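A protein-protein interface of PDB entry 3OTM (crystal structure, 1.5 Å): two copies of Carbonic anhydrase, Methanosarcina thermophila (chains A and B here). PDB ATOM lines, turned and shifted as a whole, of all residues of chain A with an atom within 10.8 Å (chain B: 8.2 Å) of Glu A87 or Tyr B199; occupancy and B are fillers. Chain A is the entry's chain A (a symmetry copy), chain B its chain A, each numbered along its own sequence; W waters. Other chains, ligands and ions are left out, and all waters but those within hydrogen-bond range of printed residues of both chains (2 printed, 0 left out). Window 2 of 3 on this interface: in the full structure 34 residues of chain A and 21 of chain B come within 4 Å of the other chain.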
ATOM      1  N   VAL A  15     -19.569  24.686 -27.034  1.00  0.00           N
ATOM      2  CA  VAL A  15     -19.480  24.165 -28.393  1.00  0.00           C
ATOM      3  C   VAL A  15     -19.950  22.718 -28.382  1.00  0.00           C
ATOM      4  O   VAL A  15     -19.509  21.908 -27.556  1.00  0.00           O
ATOM      5  CB  VAL A  15     -18.040  24.256 -28.948  1.00  0.00           C
ATOM      6  CG1 VAL A  15     -17.981  23.627 -30.332  1.00  0.00           C
ATOM      7  CG2 VAL A  15     -17.591  25.707 -28.986  1.00  0.00           C
ATOM      8  N   THR A  16     -20.886  22.412 -29.272  1.00  0.00           N
ATOM      9  CA  THR A  16     -21.420  21.070 -29.431  1.00  0.00           C
ATOM     10  C   THR A  16     -21.652  20.804 -30.901  1.00  0.00           C
ATOM     11  O   THR A  16     -21.483  21.694 -31.733  1.00  0.00           O
ATOM     12  CB  THR A  16     -22.791  20.933 -28.776  1.00  0.00           C
ATOM     13  OG1 THR A  16     -23.716  21.787 -29.452  1.00  0.00           O
ATOM     14  CG2 THR A  16     -22.731  21.327 -27.289  1.00  0.00           C
ATOM     15  N   PRO A  17     -22.074  19.579 -31.233  1.00  0.00           N
ATOM     16  CA  PRO A  17     -22.274  19.366 -32.675  1.00  0.00           C
ATOM     17  C   PRO A  17     -23.430  20.164 -33.298  1.00  0.00           C
ATOM     18  O   PRO A  17     -23.481  20.302 -34.516  1.00  0.00           O
ATOM     19  CB  PRO A  17     -22.502  17.853 -32.795  1.00  0.00           C
ATOM     20  CG  PRO A  17     -22.511  17.298 -31.414  1.00  0.00           C
ATOM     21  CD  PRO A  17     -22.000  18.326 -30.461  1.00  0.00           C
ATOM     22  N   TRP A  18     -24.323  20.704 -32.482  1.00  0.00           N
ATOM     23  CA  TRP A  18     -25.431  21.525 -32.986  1.00  0.00           C
ATOM     24  C   TRP A  18     -25.228  22.999 -32.702  1.00  0.00           C
ATOM     25  O   TRP A  18     -26.125  23.806 -32.958  1.00  0.00           O
ATOM     26  CB  TRP A  18     -26.747  21.110 -32.346  1.00  0.00           C
ATOM     27  CG  TRP A  18     -26.730  21.213 -30.848  1.00  0.00           C
ATOM     28  CD1 TRP A  18     -27.024  22.314 -30.091  1.00  0.00           C
ATOM     29  CD2 TRP A  18     -26.406  20.168 -29.929  1.00  0.00           C
ATOM     30  NE1 TRP A  18     -26.905  22.012 -28.758  1.00  0.00           N
ATOM     31  CE2 TRP A  18     -26.533  20.701 -28.628  1.00  0.00           C
ATOM     32  CE3 TRP A  18     -26.038  18.829 -30.078  1.00  0.00           C
ATOM     33  CZ2 TRP A  18     -26.277  19.952 -27.485  1.00  0.00           C
ATOM     34  CZ3 TRP A  18     -25.787  18.081 -28.935  1.00  0.00           C
ATOM     35  CH2 TRP A  18     -25.919  18.645 -27.659  1.00  0.00           C
ATOM     36  N   ASN A  19     -24.064  23.344 -32.161  1.00  0.00           N
ATOM     37  CA  ASN A  19     -23.750  24.716 -31.770  1.00  0.00           C
ATOM     38  C   ASN A  19     -22.282  25.008 -32.041  1.00  0.00           C
ATOM     39  O   ASN A  19     -21.451  24.928 -31.145  1.00  0.00           O
ATOM     40  CB  ASN A  19     -24.053  24.952 -30.283  1.00  0.00           C
ATOM     41  CG  ASN A  19     -23.994  26.418 -29.908  1.00  0.00           C
ATOM     42  OD1 ASN A  19     -24.611  27.250 -30.555  1.00  0.00           O
ATOM     43  ND2 ASN A  19     -23.249  26.743 -28.866  1.00  0.00           N
ATOM     44  N   PRO A  20     -21.955  25.350 -33.289  1.00  0.00           N
ATOM     45  CA  PRO A  20     -20.581  25.604 -33.727  1.00  0.00           C
ATOM     46  C   PRO A  20     -19.951  26.821 -33.054  1.00  0.00           C
ATOM     47  O   PRO A  20     -18.734  26.861 -32.871  1.00  0.00           O
ATOM     48  CB  PRO A  20     -20.742  25.868 -35.232  1.00  0.00           C
ATOM     49  CG  PRO A  20     -22.085  25.290 -35.598  1.00  0.00           C
ATOM     50  CD  PRO A  20     -22.925  25.446 -34.393  1.00  0.00           C
ATOM     51  N   ASP A  60     -28.958  25.994 -24.409  1.00  0.00           N
ATOM     52  CA  ASP A  60     -27.775  25.258 -24.859  1.00  0.00           C
ATOM     53  C   ASP A  60     -28.099  24.145 -25.836  1.00  0.00           C
ATOM     54  O   ASP A  60     -27.224  23.410 -26.264  1.00  0.00           O
ATOM     55  CB  ASP A  60     -26.939  24.735 -23.678  1.00  0.00           C
ATOM     56  CG  ASP A  60     -27.730  23.883 -22.699  1.00  0.00           C
ATOM     57  OD1 ASP A  60     -27.121  23.510 -21.688  1.00  0.00           O
ATOM     58  OD2 ASP A  60     -28.898  23.580 -22.979  1.00  0.00           O
ATOM     59  N   GLU A  61     -29.320  24.145 -26.365  1.00  0.00           N
ATOM     60  CA  GLU A  61     -29.670  23.157 -27.389  1.00  0.00           C
ATOM     61  C   GLU A  61     -30.112  23.747 -28.725  1.00  0.00           C
ATOM     62  O   GLU A  61     -30.805  23.083 -29.502  1.00  0.00           O
ATOM     63  CB  GLU A  61     -30.728  22.205 -26.857  1.00  0.00           C
ATOM     64  CG  GLU A  61     -30.347  21.574 -25.522  1.00  0.00           C
ATOM     65  CD  GLU A  61     -31.056  20.269 -25.292  1.00  0.00           C
ATOM     66  OE1 GLU A  61     -31.086  19.747 -24.157  1.00  0.00           O
ATOM     67  OE2 GLU A  61     -31.602  19.752 -26.257  1.00  0.00           O
ATOM     68  N   GLY A  62     -29.680  24.976 -29.013  1.00  0.00           N
ATOM     69  CA  GLY A  62     -30.004  25.641 -30.268  1.00  0.00           C
ATOM     70  C   GLY A  62     -31.212  26.556 -30.162  1.00  0.00           C
ATOM     71  O   GLY A  62     -32.151  26.272 -29.422  1.00  0.00           O
ATOM     72  N   GLU A  83     -33.894  20.090 -28.429  1.00  0.00           N
ATOM     73  CA  GLU A  83     -33.002  20.455 -29.527  1.00  0.00           C
ATOM     74  C   GLU A  83     -33.770  20.970 -30.745  1.00  0.00           C
ATOM     75  O   GLU A  83     -34.783  20.398 -31.165  1.00  0.00           O
ATOM     76  CB  GLU A  83     -32.128  19.242 -29.886  1.00  0.00           C
ATOM     77  CG  GLU A  83     -31.038  19.532 -30.899  1.00  0.00           C
ATOM     78  CD  GLU A  83     -30.118  18.336 -31.119  1.00  0.00           C
ATOM     79  OE1 GLU A  83     -30.359  17.279 -30.503  1.00  0.00           O
ATOM     80  OE2 GLU A  83     -29.154  18.454 -31.903  1.00  0.00           O
ATOM     81  N   THR A  84     -33.287  22.069 -31.303  1.00  0.00           N
ATOM     82  CA  THR A  84     -33.944  22.744 -32.412  1.00  0.00           C
ATOM     83  C   THR A  84     -33.173  22.561 -33.709  1.00  0.00           C
ATOM     84  O   THR A  84     -33.690  22.847 -34.782  1.00  0.00           O
ATOM     85  CB  THR A  84     -34.094  24.242 -32.135  1.00  0.00           C
ATOM     86  OG1 THR A  84     -32.827  24.787 -31.715  1.00  0.00           O
ATOM     87  CG2 THR A  84     -35.131  24.457 -31.049  1.00  0.00           C
ATOM     88  N   ILE A  85     -31.934  22.100 -33.585  1.00  0.00           N
ATOM     89  CA  ILE A  85     -31.065  21.821 -34.734  1.00  0.00           C
ATOM     90  C   ILE A  85     -30.400  20.474 -34.481  1.00  0.00           C
ATOM     91  O   ILE A  85     -29.768  20.306 -33.444  1.00  0.00           O
ATOM     92  CB  ILE A  85     -29.935  22.872 -34.856  1.00  0.00           C
ATOM     93  CG1 ILE A  85     -30.509  24.289 -34.949  1.00  0.00           C
ATOM     94  CG2 ILE A  85     -29.051  22.573 -36.059  1.00  0.00           C
ATOM     95  CD1 ILE A  85     -31.167  24.602 -36.283  1.00  0.00           C
ATOM     96  N   ASN A  86     -30.537  19.506 -35.384  1.00  0.00           N
ATOM     97  CA  ASN A  86     -29.857  18.224 -35.179  1.00  0.00           C
ATOM     98  C   ASN A  86     -28.391  18.294 -35.624  1.00  0.00           C
ATOM     99  O   ASN A  86     -27.938  19.327 -36.116  1.00  0.00           O
ATOM    100  CB  ASN A  86     -30.609  17.054 -35.837  1.00  0.00           C
ATOM    101  CG  ASN A  86     -30.599  17.109 -37.356  1.00  0.00           C
ATOM    102  OD1 ASN A  86     -29.746  17.749 -37.972  1.00  0.00           O
ATOM    103  ND2 ASN A  86     -31.555  16.417 -37.970  1.00  0.00           N
ATOM    104  N   GLU A  87     -27.649  17.210 -35.427  1.00  0.00           N
ATOM    105  CA  GLU A  87     -26.211  17.216 -35.686  1.00  0.00           C
ATOM    106  C   GLU A  87     -25.877  17.539 -37.137  1.00  0.00           C
ATOM    107  O   GLU A  87     -24.822  18.101 -37.427  1.00  0.00           O
ATOM    108  CB  GLU A  87     -25.595  15.870 -35.311  1.00  0.00           C
ATOM    109  CG  GLU A  87     -25.425  15.670 -33.821  1.00  0.00           C
ATOM    110  CD  GLU A  87     -24.668  14.405 -33.499  1.00  0.00           C
ATOM    111  OE1 GLU A  87     -25.265  13.318 -33.617  1.00  0.00           O
ATOM    112  OE2 GLU A  87     -23.475  14.498 -33.140  1.00  0.00           O
ATOM    113  N   GLU A  88     -26.781  17.186 -38.044  1.00  0.00           N
ATOM    114  CA  GLU A  88     -26.548  17.374 -39.468  1.00  0.00           C
ATOM    115  C   GLU A  88     -26.948  18.777 -39.929  1.00  0.00           C
ATOM    116  O   GLU A  88     -27.074  19.034 -41.127  1.00  0.00           O
ATOM    117  CB  GLU A  88     -27.307  16.306 -40.256  1.00  0.00           C
ATOM    118  CG  GLU A  88     -27.008  14.889 -39.780  1.00  0.00           C
ATOM    119  CD  GLU A  88     -27.840  13.839 -40.490  1.00  0.00           C
ATOM    120  OE1 GLU A  88     -28.708  14.212 -41.304  1.00  0.00           O
ATOM    121  OE2 GLU A  88     -27.623  12.637 -40.233  1.00  0.00           O
ATOM    122  N   GLY A  89     -27.139  19.680 -38.971  1.00  0.00           N
ATOM    123  CA  GLY A  89     -27.432  21.073 -39.264  1.00  0.00           C
ATOM    124  C   GLY A  89     -28.878  21.340 -39.636  1.00  0.00           C
ATOM    125  O   GLY A  89     -29.252  22.479 -39.918  1.00  0.00           O
ATOM    126  N   GLU A  90     -29.697  20.294 -39.630  1.00  0.00           N
ATOM    127  CA  GLU A  90     -31.087  20.411 -40.057  1.00  0.00           C
ATOM    128  C   GLU A  90     -31.996  20.868 -38.918  1.00  0.00           C
ATOM    129  O   GLU A  90     -32.038  20.240 -37.864  1.00  0.00           O
ATOM    130  CB  GLU A  90     -31.580  19.073 -40.604  1.00  0.00           C
ATOM    131  CG  GLU A  90     -30.846  18.614 -41.852  1.00  0.00           C
ATOM    132  CD  GLU A  90     -31.340  17.274 -42.358  1.00  0.00           C
ATOM    133  OE1 GLU A  90     -31.943  16.522 -41.563  1.00  0.00           O
ATOM    134  OE2 GLU A  90     -31.128  16.973 -43.551  1.00  0.00           O
ATOM    135  N   PRO A  91     -32.731  21.967 -39.132  1.00  0.00           N
ATOM    136  CA  PRO A  91     -33.671  22.453 -38.116  1.00  0.00           C
ATOM    137  C   PRO A  91     -34.832  21.482 -37.871  1.00  0.00           C
ATOM    138  O   PRO A  91     -35.454  21.005 -38.819  1.00  0.00           O
ATOM    139  CB  PRO A  91     -34.173  23.777 -38.705  1.00  0.00           C
ATOM    140  CG  PRO A  91     -33.920  23.676 -40.165  1.00  0.00           C
ATOM    141  CD  PRO A  91     -32.694  22.840 -40.317  1.00  0.00           C
ATOM    142  N   ILE A  92     -35.102  21.187 -36.601  1.00  0.00           N
ATOM    143  CA  ILE A  92     -36.203  20.311 -36.210  1.00  0.00           C
ATOM    144  C   ILE A  92     -37.488  21.130 -35.986  1.00  0.00           C
ATOM    145  O   ILE A  92     -37.733  21.637 -34.890  1.00  0.00           O
ATOM    146  CB  ILE A  92     -35.840  19.550 -34.918  1.00  0.00           C
ATOM    147  CG1 ILE A  92     -34.489  18.838 -35.077  1.00  0.00           C
ATOM    148  CG2 ILE A  92     -36.942  18.572 -34.555  1.00  0.00           C
ATOM    149  CD1 ILE A  92     -33.990  18.154 -33.810  1.00  0.00           C
ATOM    150  N   ASN B  48     -19.306  10.553 -17.713  1.00  0.00           N
ATOM    151  CA  ASN B  48     -20.059  11.330 -18.690  1.00  0.00           C
ATOM    152  C   ASN B  48     -21.391  11.848 -18.170  1.00  0.00           C
ATOM    153  O   ASN B  48     -22.300  12.120 -18.954  1.00  0.00           O
ATOM    154  CB  ASN B  48     -20.290  10.507 -19.963  1.00  0.00           C
ATOM    155  CG  ASN B  48     -18.991  10.050 -20.586  1.00  0.00           C
ATOM    156  OD1 ASN B  48     -18.201  10.871 -21.031  1.00  0.00           O
ATOM    157  ND2 ASN B  48     -18.739   8.756 -20.543  1.00  0.00           N
ATOM    158  N   ARG B  70     -23.430   7.895 -17.853  1.00  0.00           N
ATOM    159  CA  ARG B  70     -24.189   8.521 -18.932  1.00  0.00           C
ATOM    160  C   ARG B  70     -25.598   8.953 -18.527  1.00  0.00           C
ATOM    161  O   ARG B  70     -26.465   9.141 -19.369  1.00  0.00           O
ATOM    162  CB  ARG B  70     -24.246   7.611 -20.166  1.00  0.00           C
ATOM    163  CG  ARG B  70     -22.874   7.329 -20.769  1.00  0.00           C
ATOM    164  CD  ARG B  70     -22.907   6.239 -21.862  1.00  0.00           C
ATOM    165  NE  ARG B  70     -23.547   5.037 -21.361  1.00  0.00           N
ATOM    166  CZ  ARG B  70     -22.921   4.060 -20.712  1.00  0.00           C
ATOM    167  NH1 ARG B  70     -21.601   4.092 -20.538  1.00  0.00           N
ATOM    168  NH2 ARG B  70     -23.611   3.029 -20.270  1.00  0.00           N
ATOM    169  N   ASN B  72     -28.056  11.839 -16.420  1.00  0.00           N
ATOM    170  CA  ASN B  72     -28.064  13.269 -16.292  1.00  0.00           C
ATOM    171  C   ASN B  72     -28.985  13.706 -15.170  1.00  0.00           C
ATOM    172  O   ASN B  72     -30.019  13.084 -14.915  1.00  0.00           O
ATOM    173  CB  ASN B  72     -28.419  13.984 -17.624  1.00  0.00           C
ATOM    174  CG  ASN B  72     -29.743  13.553 -18.211  1.00  0.00           C
ATOM    175  OD1 ASN B  72     -30.789  14.069 -17.844  1.00  0.00           O
ATOM    176  ND2 ASN B  72     -29.699  12.609 -19.137  1.00  0.00           N
ATOM    177  N   ASN B 111     -27.623   5.581 -18.116  1.00  0.00           N
ATOM    178  CA  ASN B 111     -28.452   6.167 -19.179  1.00  0.00           C
ATOM    179  C   ASN B 111     -29.821   6.600 -18.683  1.00  0.00           C
ATOM    180  O   ASN B 111     -30.825   6.418 -19.379  1.00  0.00           O
ATOM    181  CB  ASN B 111     -28.666   5.199 -20.339  1.00  0.00           C
ATOM    182  CG  ASN B 111     -27.386   4.561 -20.817  1.00  0.00           C
ATOM    183  OD1 ASN B 111     -26.396   5.221 -21.072  1.00  0.00           O
ATOM    184  ND2 ASN B 111     -27.442   3.265 -21.021  1.00  0.00           N
ATOM    185  N   SER B 113     -32.284   9.716 -17.382  1.00  0.00           N
ATOM    186  CA  SER B 113     -32.468  11.153 -17.369  1.00  0.00           C
ATOM    187  C   SER B 113     -33.365  11.562 -16.213  1.00  0.00           C
ATOM    188  O   SER B 113     -34.504  11.079 -16.101  1.00  0.00           O
ATOM    189  CB  SER B 113     -33.141  11.611 -18.651  1.00  0.00           C
ATOM    190  OG  SER B 113     -32.358  11.281 -19.795  1.00  0.00           O
ATOM    191  N   HIS B 192     -38.845   7.370 -27.632  1.00  0.00           N
ATOM    192  CA  HIS B 192     -37.445   7.642 -27.994  1.00  0.00           C
ATOM    193  C   HIS B 192     -36.856   8.840 -27.271  1.00  0.00           C
ATOM    194  O   HIS B 192     -35.749   9.263 -27.564  1.00  0.00           O
ATOM    195  CB  HIS B 192     -37.333   7.880 -29.502  1.00  0.00           C
ATOM    196  CG  HIS B 192     -37.838   6.737 -30.319  1.00  0.00           C
ATOM    197  ND1 HIS B 192     -38.621   6.914 -31.439  1.00  0.00           N
ATOM    198  CD2 HIS B 192     -37.686   5.400 -30.172  1.00  0.00           C
ATOM    199  CE1 HIS B 192     -38.927   5.735 -31.949  1.00  0.00           C
ATOM    200  NE2 HIS B 192     -38.375   4.800 -31.197  1.00  0.00           N
ATOM    201  N   THR B 193     -37.582   9.378 -26.306  1.00  0.00           N
ATOM    202  CA  THR B 193     -37.185  10.601 -25.646  1.00  0.00           C
ATOM    203  C   THR B 193     -35.909  10.397 -24.859  1.00  0.00           C
ATOM    204  O   THR B 193     -34.992  11.201 -24.966  1.00  0.00           O
ATOM    205  CB  THR B 193     -38.318  11.124 -24.737  1.00  0.00           C
ATOM    206  OG1 THR B 193     -39.446  11.455 -25.557  1.00  0.00           O
ATOM    207  CG2 THR B 193     -37.904  12.354 -23.915  1.00  0.00           C
ATOM    208  N   ASN B 194     -35.811   9.309 -24.110  1.00  0.00           N
ATOM    209  CA  ASN B 194     -34.659   9.163 -23.236  1.00  0.00           C
ATOM    210  C   ASN B 194     -33.360   9.035 -24.023  1.00  0.00           C
ATOM    211  O   ASN B 194     -32.355   9.624 -23.633  1.00  0.00           O
ATOM    212  CB  ASN B 194     -34.795   7.983 -22.305  1.00  0.00           C
ATOM    213  CG  ASN B 194     -33.808   8.066 -21.173  1.00  0.00           C
ATOM    214  OD1 ASN B 194     -33.832   9.034 -20.410  1.00  0.00           O
ATOM    215  ND2 ASN B 194     -32.911   7.116 -21.100  1.00  0.00           N
ATOM    216  N   GLU B 195     -33.375   8.274 -25.119  1.00  0.00           N
ATOM    217  CA  GLU B 195     -32.169   8.076 -25.908  1.00  0.00           C
ATOM    218  C   GLU B 195     -31.677   9.407 -26.465  1.00  0.00           C
ATOM    219  O   GLU B 195     -30.463   9.656 -26.521  1.00  0.00           O
ATOM    220  CB  GLU B 195     -32.418   7.084 -27.060  1.00  0.00           C
ATOM    221  CG  GLU B 195     -32.765   5.696 -26.595  1.00  0.00           C
ATOM    222  CD  GLU B 195     -32.512   4.645 -27.655  1.00  0.00           C
ATOM    223  OE1 GLU B 195     -32.256   5.019 -28.823  1.00  0.00           O
ATOM    224  OE2 GLU B 195     -32.562   3.443 -27.307  1.00  0.00           O
ATOM    225  N   ALA B 196     -32.612  10.257 -26.878  1.00  0.00           N
ATOM    226  CA  ALA B 196     -32.248  11.571 -27.414  1.00  0.00           C
ATOM    227  C   ALA B 196     -31.652  12.445 -26.328  1.00  0.00           C
ATOM    228  O   ALA B 196     -30.631  13.118 -26.551  1.00  0.00           O
ATOM    229  CB  ALA B 196     -33.480  12.254 -28.036  1.00  0.00           C
ATOM    230  N   VAL B 197     -32.259  12.433 -25.146  1.00  0.00           N
ATOM    231  CA  VAL B 197     -31.822  13.286 -24.045  1.00  0.00           C
ATOM    232  C   VAL B 197     -30.445  12.820 -23.539  1.00  0.00           C
ATOM    233  O   VAL B 197     -29.586  13.638 -23.221  1.00  0.00           O
ATOM    234  CB  VAL B 197     -32.871  13.300 -22.910  1.00  0.00           C
ATOM    235  CG1 VAL B 197     -32.389  14.053 -21.689  1.00  0.00           C
ATOM    236  CG2 VAL B 197     -34.173  13.919 -23.420  1.00  0.00           C
ATOM    237  N   VAL B 198     -30.213  11.520 -23.492  1.00  0.00           N
ATOM    238  CA  VAL B 198     -28.920  11.000 -23.065  1.00  0.00           C
ATOM    239  C   VAL B 198     -27.858  11.407 -24.071  1.00  0.00           C
ATOM    240  O   VAL B 198     -26.771  11.867 -23.701  1.00  0.00           O
ATOM    241  CB  VAL B 198     -28.978   9.476 -22.889  1.00  0.00           C
ATOM    242  CG1 VAL B 198     -27.561   8.874 -22.801  1.00  0.00           C
ATOM    243  CG2 VAL B 198     -29.750   9.156 -21.640  1.00  0.00           C
ATOM    244  N   TYR B 199     -28.137  11.235 -25.357  1.00  0.00           N
ATOM    245  CA  TYR B 199     -27.170  11.639 -26.379  1.00  0.00           C
ATOM    246  C   TYR B 199     -26.797  13.121 -26.230  1.00  0.00           C
ATOM    247  O   TYR B 199     -25.604  13.479 -26.278  1.00  0.00           O
ATOM    248  CB  TYR B 199     -27.742  11.369 -27.771  1.00  0.00           C
ATOM    249  CG  TYR B 199     -26.753  11.499 -28.891  1.00  0.00           C
ATOM    250  CD1 TYR B 199     -25.926  10.440 -29.251  1.00  0.00           C
ATOM    251  CD2 TYR B 199     -26.669  12.662 -29.604  1.00  0.00           C
ATOM    252  CE1 TYR B 199     -25.034  10.559 -30.305  1.00  0.00           C
ATOM    253  CE2 TYR B 199     -25.756  12.799 -30.656  1.00  0.00           C
ATOM    254  CZ  TYR B 199     -24.961  11.741 -30.997  1.00  0.00           C
ATOM    255  OH  TYR B 199     -24.074  11.850 -32.043  1.00  0.00           O
ATOM    256  N   VAL B 200     -27.805  13.974 -26.060  1.00  0.00           N
ATOM    257  CA  VAL B 200     -27.559  15.407 -25.926  1.00  0.00           C
ATOM    258  C   VAL B 200     -26.745  15.691 -24.683  1.00  0.00           C
ATOM    259  O   VAL B 200     -25.788  16.470 -24.735  1.00  0.00           O
ATOM    260  CB  VAL B 200     -28.887  16.193 -25.891  1.00  0.00           C
ATOM    261  CG1 VAL B 200     -28.658  17.615 -25.421  1.00  0.00           C
ATOM    262  CG2 VAL B 200     -29.527  16.156 -27.283  1.00  0.00           C
ATOM    263  N   ASN B 201     -27.099  15.092 -23.557  1.00  0.00           N
ATOM    264  CA  ASN B 201     -26.429  15.424 -22.321  1.00  0.00           C
ATOM    265  C   ASN B 201     -25.008  14.920 -22.227  1.00  0.00           C
ATOM    266  O   ASN B 201     -24.184  15.573 -21.593  1.00  0.00           O
ATOM    267  CB  ASN B 201     -27.231  14.992 -21.081  1.00  0.00           C
ATOM    268  CG  ASN B 201     -28.309  15.980 -20.723  1.00  0.00           C
ATOM    269  OD1 ASN B 201     -28.104  16.884 -19.901  1.00  0.00           O
ATOM    270  ND2 ASN B 201     -29.463  15.803 -21.311  1.00  0.00           N
ATOM    271  N   VAL B 202     -24.699  13.776 -22.842  1.00  0.00           N
ATOM    272  CA  VAL B 202     -23.308  13.327 -22.895  1.00  0.00           C
ATOM    273  C   VAL B 202     -22.487  14.334 -23.675  1.00  0.00           C
ATOM    274  O   VAL B 202     -21.345  14.638 -23.299  1.00  0.00           O
ATOM    275  CB  VAL B 202     -23.235  11.912 -23.498  1.00  0.00           C
ATOM    276  CG1 VAL B 202     -21.820  11.546 -23.894  1.00  0.00           C
ATOM    277  CG2 VAL B 202     -23.789  10.935 -22.477  1.00  0.00           C
ATOM    278  N   HIS B 203     -23.045  14.872 -24.753  1.00  0.00           N
ATOM    279  CA  HIS B 203     -22.325  15.906 -25.510  1.00  0.00           C
ATOM    280  C   HIS B 203     -22.236  17.250 -24.801  1.00  0.00           C
ATOM    281  O   HIS B 203     -21.223  17.964 -24.935  1.00  0.00           O
ATOM    282  CB  HIS B 203     -22.934  16.072 -26.891  1.00  0.00           C
ATOM    283  CG  HIS B 203     -22.603  14.944 -27.809  1.00  0.00           C
ATOM    284  ND1 HIS B 203     -23.254  13.731 -27.759  1.00  0.00           N
ATOM    285  CD2 HIS B 203     -21.654  14.828 -28.767  1.00  0.00           C
ATOM    286  CE1 HIS B 203     -22.721  12.917 -28.653  1.00  0.00           C
ATOM    287  NE2 HIS B 203     -21.758  13.562 -29.286  1.00  0.00           N
ATOM    288  N   LEU B 204     -23.280  17.622 -24.070  1.00  0.00           N
ATOM    289  CA  LEU B 204     -23.203  18.836 -23.249  1.00  0.00           C
ATOM    290  C   LEU B 204     -22.135  18.723 -22.172  1.00  0.00           C
ATOM    291  O   LEU B 204     -21.405  19.684 -21.907  1.00  0.00           O
ATOM    292  CB  LEU B 204     -24.562  19.156 -22.601  1.00  0.00           C
ATOM    293  CG  LEU B 204     -25.616  19.756 -23.504  1.00  0.00           C
ATOM    294  CD1 LEU B 204     -26.942  19.869 -22.746  1.00  0.00           C
ATOM    295  CD2 LEU B 204     -25.159  21.105 -24.006  1.00  0.00           C
ATOM    296  N   ALA B 205     -22.033  17.572 -21.511  1.00  0.00           N
ATOM    297  CA  ALA B 205     -21.045  17.401 -20.462  1.00  0.00           C
ATOM    298  C   ALA B 205     -19.642  17.646 -21.038  1.00  0.00           C
ATOM    299  O   ALA B 205     -18.834  18.345 -20.425  1.00  0.00           O
ATOM    300  CB  ALA B 205     -21.161  16.016 -19.836  1.00  0.00           C
HETATM  301  O   HOH W   1     -31.509  17.988 -21.941  1.00  0.00           O
HETATM  302  O   HOH W   2     -19.844  18.704 -27.237  1.00  0.00           O
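The side-chain carboxylate (OE1) of Glu A87 sits at hydrogen-bond distance from the side-chain hydroxyl (OH) of Tyr B199, 2.5 Å away.
A ring nitrogen (ND1) of His B203 is in hydrogen-bond range of the backbone carbonyl oxygen (O) of Tyr B199 (2.8 Å).
The indole nitrogen (NE1) of Trp A18 sits close to the side-chain hydroxyl (OG1) of Thr A16 (3.3 Å).
O of Asp A60 sits at hydrogen-bond distance from NE1 of Trp A18 (2.9 Å).
OE2 of Glu A61 is in hydrogen-bond range of N of Glu A83 (3.2 Å).
The backbone carbonyl oxygen (O) of Glu A61 sits at hydrogen-bond distance from the backbone NH (N) of Thr A84, at 3.2 Å.
OE2 of Glu A83 sits close to O of Ile A85 (2.5 Å).
Printed residues of chain B within 4 Å of Pro A17: His B203 (3.7 Å).
Printed residues of chain B within 4 Å of Trp A18: Val B200 (3.6 Å) and Leu B204 (3.8 Å).
Of the printed residues of chain B, Glu A61 touches Val B200.
Of chain B, only Tyr B199 comes within 4 Å of Glu A87.
No residue of chain A comes within 4 Å of Ala B196.
No residue of chain A comes within 4 Å of Val B198.
Of chain A, only Glu A87 (2.5 Å) comes within 4 Å of Tyr B199.
No residue of chain A comes within 4 Å of Val B202.
Printed residues of chain A within 4 Å of Leu B204: Trp A18 and Asp A60.
The nearest residue of chain A that does not touch Tyr B199 is Trp A18 (5.3 Å).
The nearest printed residue of chain B that does not touch Pro A17 is Tyr B199 (5.6 Å).
No position is printed for both chains.
Among the printed residues, pairs that only touch across the chains: Pro A17 with His B203, Trp A18 with Val B200, Trp A18 with Leu B204, Asp A60 with Leu B204, Glu A61 with Val B200 and Glu A83 with Val B200.
Water W2 bridges O of His B203 and O of Val A15.
Water W1 lies within hydrogen-bond range of OE1 of Glu A61 and ND2 of Asn B201.
Hydrophobic or aromatic side chains of chain B that line the printed part of chain A: Tyr B199, Val B200, His B203 and Leu B204.
Of the 19 printed residues of chain A, 6 touch a printed residue of chain B.
Printed residues of chain A that touch a printed residue of chain B: Pro A17, Trp A18, Asp A60, Glu A61, Glu A83 and Glu A87.
Hydrophobic or aromatic side chains of chain A within 4 Å of the printed part of chain B: Pro A17 and Trp A18.
Among the printed residues, 7 pairs touch across the chains.
Among the printed residues, no Asp or Glu carboxylate lies within 4 Å of a Lys or Arg side-chain nitrogen of the other chain.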
